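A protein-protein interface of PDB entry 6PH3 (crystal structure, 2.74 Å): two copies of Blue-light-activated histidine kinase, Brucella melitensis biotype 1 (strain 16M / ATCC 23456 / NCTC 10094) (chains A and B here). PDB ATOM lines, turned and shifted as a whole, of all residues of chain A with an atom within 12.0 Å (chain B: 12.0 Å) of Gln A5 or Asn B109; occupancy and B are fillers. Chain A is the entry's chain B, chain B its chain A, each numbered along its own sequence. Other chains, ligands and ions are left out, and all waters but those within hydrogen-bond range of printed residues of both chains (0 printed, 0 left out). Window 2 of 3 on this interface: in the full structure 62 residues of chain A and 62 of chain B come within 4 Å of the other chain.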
ATOM      1  N   SER A   4       8.661   9.180  11.197  1.00  0.00           N
ATOM      2  CA  SER A   4       7.472   9.268  10.348  1.00  0.00           C
ATOM      3  C   SER A   4       6.368  10.159  10.942  1.00  0.00           C
ATOM      4  O   SER A   4       5.667  10.839  10.185  1.00  0.00           O
ATOM      5  CB  SER A   4       6.916   7.877  10.034  1.00  0.00           C
ATOM      6  OG  SER A   4       6.130   7.336  11.086  1.00  0.00           O
ATOM      7  N   GLN A   5       6.194  10.135  12.279  1.00  0.00           N
ATOM      8  CA  GLN A   5       5.138  10.912  12.936  1.00  0.00           C
ATOM      9  C   GLN A   5       5.654  12.088  13.792  1.00  0.00           C
ATOM     10  O   GLN A   5       4.984  13.128  13.856  1.00  0.00           O
ATOM     11  CB  GLN A   5       4.219   9.982  13.761  1.00  0.00           C
ATOM     12  CG  GLN A   5       2.718  10.187  13.510  1.00  0.00           C
ATOM     13  CD  GLN A   5       2.322   9.965  12.067  1.00  0.00           C
ATOM     14  OE1 GLN A   5       2.385   8.843  11.535  1.00  0.00           O
ATOM     15  NE2 GLN A   5       1.937  11.049  11.399  1.00  0.00           N
ATOM     16  N   ALA A   6       6.832  11.918  14.444  1.00  0.00           N
ATOM     17  CA  ALA A   6       7.445  12.924  15.319  1.00  0.00           C
ATOM     18  C   ALA A   6       8.122  14.086  14.558  1.00  0.00           C
ATOM     19  O   ALA A   6       9.268  13.952  14.099  1.00  0.00           O
ATOM     20  CB  ALA A   6       8.415  12.264  16.303  1.00  0.00           C
ATOM     21  N   THR A   7       7.375  15.225  14.415  1.00  0.00           N
ATOM     22  CA  THR A   7       7.820  16.498  13.814  1.00  0.00           C
ATOM     23  C   THR A   7       8.837  17.110  14.793  1.00  0.00           C
ATOM     24  O   THR A   7       8.634  17.028  16.015  1.00  0.00           O
ATOM     25  CB  THR A   7       6.611  17.448  13.605  1.00  0.00           C
ATOM     26  OG1 THR A   7       5.649  16.805  12.776  1.00  0.00           O
ATOM     27  CG2 THR A   7       6.992  18.780  12.971  1.00  0.00           C
ATOM     28  N   ASP A   8       9.938  17.697  14.269  1.00  0.00           N
ATOM     29  CA  ASP A   8      10.964  18.281  15.129  1.00  0.00           C
ATOM     30  C   ASP A   8      10.479  19.561  15.839  1.00  0.00           C
ATOM     31  O   ASP A   8      10.116  20.527  15.142  1.00  0.00           O
ATOM     32  CB  ASP A   8      12.275  18.526  14.361  1.00  0.00           C
ATOM     33  CG  ASP A   8      13.475  18.827  15.252  1.00  0.00           C
ATOM     34  OD1 ASP A   8      13.574  18.219  16.356  1.00  0.00           O
ATOM     35  OD2 ASP A   8      14.340  19.626  14.832  1.00  0.00           O
ATOM     36  N   PRO A   9      10.467  19.593  17.211  1.00  0.00           N
ATOM     37  CA  PRO A   9      10.031  20.815  17.913  1.00  0.00           C
ATOM     38  C   PRO A   9      10.922  22.017  17.611  1.00  0.00           C
ATOM     39  O   PRO A   9      10.418  23.133  17.559  1.00  0.00           O
ATOM     40  CB  PRO A   9      10.073  20.424  19.392  1.00  0.00           C
ATOM     41  CG  PRO A   9      10.943  19.274  19.477  1.00  0.00           C
ATOM     42  CD  PRO A   9      10.840  18.534  18.174  1.00  0.00           C
ATOM     43  N   PHE A  10      12.221  21.787  17.362  1.00  0.00           N
ATOM     44  CA  PHE A  10      13.202  22.837  17.073  1.00  0.00           C
ATOM     45  C   PHE A  10      13.026  23.461  15.707  1.00  0.00           C
ATOM     46  O   PHE A  10      13.162  24.680  15.580  1.00  0.00           O
ATOM     47  CB  PHE A  10      14.626  22.324  17.269  1.00  0.00           C
ATOM     48  CG  PHE A  10      14.856  21.947  18.705  1.00  0.00           C
ATOM     49  CD1 PHE A  10      15.087  22.921  19.665  1.00  0.00           C
ATOM     50  CD2 PHE A  10      14.758  20.627  19.115  1.00  0.00           C
ATOM     51  CE1 PHE A  10      15.269  22.570  21.001  1.00  0.00           C
ATOM     52  CE2 PHE A  10      14.909  20.281  20.451  1.00  0.00           C
ATOM     53  CZ  PHE A  10      15.159  21.253  21.387  1.00  0.00           C
ATOM     54  N   ARG A  11      12.709  22.636  14.686  1.00  0.00           N
ATOM     55  CA  ARG A  11      12.444  23.092  13.324  1.00  0.00           C
ATOM     56  C   ARG A  11      11.218  24.032  13.376  1.00  0.00           C
ATOM     57  O   ARG A  11      11.253  25.105  12.789  1.00  0.00           O
ATOM     58  CB  ARG A  11      12.190  21.875  12.427  1.00  0.00           C
ATOM     59  CG  ARG A  11      11.752  22.183  10.997  1.00  0.00           C
ATOM     60  CD  ARG A  11      12.864  22.723  10.110  1.00  0.00           C
ATOM     61  NE  ARG A  11      12.374  23.161   8.798  1.00  0.00           N
ATOM     62  CZ  ARG A  11      11.786  24.335   8.567  1.00  0.00           C
ATOM     63  NH1 ARG A  11      11.575  25.187   9.563  1.00  0.00           N
ATOM     64  NH2 ARG A  11      11.386  24.655   7.340  1.00  0.00           N
ATOM     65  N   ALA A  12      10.178  23.656  14.139  1.00  0.00           N
ATOM     66  CA  ALA A  12       8.980  24.454  14.303  1.00  0.00           C
ATOM     67  C   ALA A  12       9.253  25.711  15.113  1.00  0.00           C
ATOM     68  O   ALA A  12       8.675  26.760  14.803  1.00  0.00           O
ATOM     69  CB  ALA A  12       7.905  23.629  14.977  1.00  0.00           C
ATOM     70  N   HIS B  27       0.932  17.054  26.358  1.00  0.00           N
ATOM     71  CA  HIS B  27       0.644  15.676  26.770  1.00  0.00           C
ATOM     72  C   HIS B  27       1.117  15.345  28.178  1.00  0.00           C
ATOM     73  O   HIS B  27       0.747  14.297  28.711  1.00  0.00           O
ATOM     74  CB  HIS B  27       1.182  14.673  25.759  1.00  0.00           C
ATOM     75  CG  HIS B  27       0.678  14.929  24.376  1.00  0.00           C
ATOM     76  ND1 HIS B  27      -0.676  15.142  24.120  1.00  0.00           N
ATOM     77  CD2 HIS B  27       1.364  15.048  23.217  1.00  0.00           C
ATOM     78  CE1 HIS B  27      -0.761  15.378  22.822  1.00  0.00           C
ATOM     79  NE2 HIS B  27       0.439  15.314  22.237  1.00  0.00           N
ATOM     80  N   GLU B  79      -6.103  25.404  20.442  1.00  0.00           N
ATOM     81  CA  GLU B  79      -4.913  24.925  19.720  1.00  0.00           C
ATOM     82  C   GLU B  79      -4.624  25.910  18.567  1.00  0.00           C
ATOM     83  O   GLU B  79      -4.361  25.499  17.434  1.00  0.00           O
ATOM     84  CB  GLU B  79      -5.045  23.460  19.253  1.00  0.00           C
ATOM     85  CG  GLU B  79      -5.185  22.496  20.411  1.00  0.00           C
ATOM     86  CD  GLU B  79      -5.355  21.021  20.096  1.00  0.00           C
ATOM     87  OE1 GLU B  79      -5.083  20.596  18.947  1.00  0.00           O
ATOM     88  OE2 GLU B  79      -5.740  20.280  21.029  1.00  0.00           O
ATOM     89  N   PRO B 104       1.036  26.430  18.372  1.00  0.00           N
ATOM     90  CA  PRO B 104       0.931  24.964  18.524  1.00  0.00           C
ATOM     91  C   PRO B 104       1.755  24.244  17.459  1.00  0.00           C
ATOM     92  O   PRO B 104       1.935  24.754  16.342  1.00  0.00           O
ATOM     93  CB  PRO B 104      -0.566  24.695  18.327  1.00  0.00           C
ATOM     94  CG  PRO B 104      -1.012  25.786  17.424  1.00  0.00           C
ATOM     95  CD  PRO B 104      -0.187  27.002  17.759  1.00  0.00           C
ATOM     96  N   VAL B 105       2.254  23.057  17.820  1.00  0.00           N
ATOM     97  CA  VAL B 105       3.007  22.214  16.901  1.00  0.00           C
ATOM     98  C   VAL B 105       2.177  20.963  16.699  1.00  0.00           C
ATOM     99  O   VAL B 105       1.877  20.269  17.670  1.00  0.00           O
ATOM    100  CB  VAL B 105       4.469  21.914  17.345  1.00  0.00           C
ATOM    101  CG1 VAL B 105       5.200  21.104  16.279  1.00  0.00           C
ATOM    102  CG2 VAL B 105       5.227  23.195  17.662  1.00  0.00           C
ATOM    103  N   HIS B 106       1.731  20.728  15.455  1.00  0.00           N
ATOM    104  CA  HIS B 106       0.891  19.584  15.067  1.00  0.00           C
ATOM    105  C   HIS B 106       1.635  18.729  14.069  1.00  0.00           C
ATOM    106  O   HIS B 106       2.417  19.272  13.293  1.00  0.00           O
ATOM    107  CB  HIS B 106      -0.416  20.067  14.424  1.00  0.00           C
ATOM    108  CG  HIS B 106      -1.346  20.819  15.336  1.00  0.00           C
ATOM    109  ND1 HIS B 106      -2.247  20.160  16.147  1.00  0.00           N
ATOM    110  CD2 HIS B 106      -1.558  22.150  15.450  1.00  0.00           C
ATOM    111  CE1 HIS B 106      -2.935  21.103  16.774  1.00  0.00           C
ATOM    112  NE2 HIS B 106      -2.571  22.316  16.376  1.00  0.00           N
ATOM    113  N   ASN B 107       1.394  17.401  14.049  1.00  0.00           N
ATOM    114  CA  ASN B 107       2.034  16.540  13.033  1.00  0.00           C
ATOM    115  C   ASN B 107       1.268  16.594  11.682  1.00  0.00           C
ATOM    116  O   ASN B 107       0.410  17.472  11.481  1.00  0.00           O
ATOM    117  CB  ASN B 107       2.234  15.092  13.521  1.00  0.00           C
ATOM    118  CG  ASN B 107       0.974  14.302  13.768  1.00  0.00           C
ATOM    119  OD1 ASN B 107      -0.127  14.664  13.333  1.00  0.00           O
ATOM    120  ND2 ASN B 107       1.113  13.190  14.478  1.00  0.00           N
ATOM    121  N   ALA B 108       1.586  15.645  10.764  1.00  0.00           N
ATOM    122  CA  ALA B 108       0.953  15.544   9.443  1.00  0.00           C
ATOM    123  C   ALA B 108      -0.533  15.191   9.588  1.00  0.00           C
ATOM    124  O   ALA B 108      -1.364  15.769   8.874  1.00  0.00           O
ATOM    125  CB  ALA B 108       1.667  14.498   8.606  1.00  0.00           C
ATOM    126  N   ASN B 109      -0.863  14.294  10.567  1.00  0.00           N
ATOM    127  CA  ASN B 109      -2.232  13.865  10.884  1.00  0.00           C
ATOM    128  C   ASN B 109      -3.037  15.013  11.464  1.00  0.00           C
ATOM    129  O   ASN B 109      -4.266  14.974  11.394  1.00  0.00           O
ATOM    130  CB  ASN B 109      -2.263  12.726  11.932  1.00  0.00           C
ATOM    131  CG  ASN B 109      -1.449  11.475  11.689  1.00  0.00           C
ATOM    132  OD1 ASN B 109      -0.959  10.855  12.652  1.00  0.00           O
ATOM    133  ND2 ASN B 109      -1.352  11.026  10.430  1.00  0.00           N
ATOM    134  N   GLY B 110      -2.345  15.978  12.083  1.00  0.00           N
ATOM    135  CA  GLY B 110      -2.952  17.122  12.761  1.00  0.00           C
ATOM    136  C   GLY B 110      -3.023  16.931  14.269  1.00  0.00           C
ATOM    137  O   GLY B 110      -3.756  17.636  14.968  1.00  0.00           O
ATOM    138  N   ARG B 111      -2.255  15.959  14.767  1.00  0.00           N
ATOM    139  CA  ARG B 111      -2.151  15.608  16.173  1.00  0.00           C
ATOM    140  C   ARG B 111      -1.216  16.637  16.867  1.00  0.00           C
ATOM    141  O   ARG B 111      -0.073  16.832  16.436  1.00  0.00           O
ATOM    142  CB  ARG B 111      -1.661  14.130  16.293  1.00  0.00           C
ATOM    143  CG  ARG B 111      -1.760  13.471  17.687  1.00  0.00           C
ATOM    144  CD  ARG B 111      -3.188  13.139  18.142  1.00  0.00           C
ATOM    145  NE  ARG B 111      -3.395  13.441  19.569  1.00  0.00           N
ATOM    146  CZ  ARG B 111      -4.582  13.618  20.151  1.00  0.00           C
ATOM    147  NH1 ARG B 111      -5.701  13.523  19.441  1.00  0.00           N
ATOM    148  NH2 ARG B 111      -4.658  13.897  21.447  1.00  0.00           N
ATOM    149  N   LEU B 112      -1.744  17.352  17.887  1.00  0.00           N
ATOM    150  CA  LEU B 112      -0.986  18.359  18.653  1.00  0.00           C
ATOM    151  C   LEU B 112       0.117  17.654  19.423  1.00  0.00           C
ATOM    152  O   LEU B 112      -0.210  16.793  20.219  1.00  0.00           O
ATOM    153  CB  LEU B 112      -1.921  19.092  19.632  1.00  0.00           C
ATOM    154  CG  LEU B 112      -1.270  20.091  20.614  1.00  0.00           C
ATOM    155  CD1 LEU B 112      -0.987  21.454  19.953  1.00  0.00           C
ATOM    156  CD2 LEU B 112      -2.147  20.292  21.815  1.00  0.00           C
ATOM    157  N   GLN B 113       1.396  18.009  19.210  1.00  0.00           N
ATOM    158  CA  GLN B 113       2.519  17.336  19.878  1.00  0.00           C
ATOM    159  C   GLN B 113       3.314  18.186  20.864  1.00  0.00           C
ATOM    160  O   GLN B 113       3.827  17.631  21.838  1.00  0.00           O
ATOM    161  CB  GLN B 113       3.465  16.722  18.851  1.00  0.00           C
ATOM    162  CG  GLN B 113       3.950  17.702  17.798  1.00  0.00           C
ATOM    163  CD  GLN B 113       5.078  17.099  17.037  1.00  0.00           C
ATOM    164  OE1 GLN B 113       4.892  16.159  16.254  1.00  0.00           O
ATOM    165  NE2 GLN B 113       6.281  17.598  17.303  1.00  0.00           N
ATOM    166  N   HIS B 114       3.419  19.507  20.607  1.00  0.00           N
ATOM    167  CA  HIS B 114       4.149  20.507  21.400  1.00  0.00           C
ATOM    168  C   HIS B 114       3.538  21.889  21.229  1.00  0.00           C
ATOM    169  O   HIS B 114       2.683  22.109  20.367  1.00  0.00           O
ATOM    170  CB  HIS B 114       5.617  20.625  20.906  1.00  0.00           C
ATOM    171  CG  HIS B 114       6.464  19.416  21.163  1.00  0.00           C
ATOM    172  ND1 HIS B 114       6.939  19.121  22.435  1.00  0.00           N
ATOM    173  CD2 HIS B 114       6.910  18.473  20.302  1.00  0.00           C
ATOM    174  CE1 HIS B 114       7.654  18.012  22.306  1.00  0.00           C
ATOM    175  NE2 HIS B 114       7.671  17.587  21.046  1.00  0.00           N
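Among the printed residues, pairs that only touch across the chains: Gln A5 with Asn B107, Gln A5 with Gln B113, Thr A7 with Asn B107, Pro A9 with His B114 and Ala A12 with Val B105.
Of the 13 printed residues of chain B, 5 touch a printed residue of chain A. Of the 9 printed residues of chain A, 4 touch a printed residue of chain B.
The backbone carbonyl oxygen (O) of Val B105 sits at hydrogen-bond distance from the backbone NH (N) of Gln B113. O of His B114 lies within hydrogen-bond range of N of Val B105 (2.8 Å). N of Asn B109 lies within hydrogen-bond range of OD1 of Asn B107 (2.9 Å). The side-chain amide oxygen (OD1) of Asn B107 lies within hydrogen-bond range of the backbone NH (N) of Gly B110. The backbone NH (N) of Arg B111 sits at hydrogen-bond distance from the side-chain amide oxygen (OD1) of Asn B107.
No residue of chain B comes within 4 Å of Ser A4. Of chain B, only Asn B107, Asn B109 and Gln B113 come within 4 Å of Gln A5. No residue of chain B comes within 4 Å of Ala A6. Printed residues of chain B within 4 Å of Pro A9: His B114. Of the printed residues of chain B, Ala A12 touches Val B105. Pro B104 touches none of the printed residues of chain A. Printed residues of chain A within 4 Å of Val B105: Ala A12 (3.8 Å). Asn B107 touches two residues of chain A. Gly B110 touches none of the printed residues of chain A. Printed residues of chain A within 4 Å of Gln B113: Gln A5 (3.9 Å) and Thr A7 (2.7 Å). The nearest residue of chain A that does not touch Asn B109 is Ser A4 (7.0 Å). The nearest printed residue of chain B that does not touch Pro A9 is Gln B113 (4.6 Å).
OD1 of Asn B109 lies within hydrogen-bond range of NE2 of Gln A5, 3.2 Å away. NE2 of Gln B113 is in hydrogen-bond range of O of Thr A7 (2.7 Å).
No position is printed for both chains.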
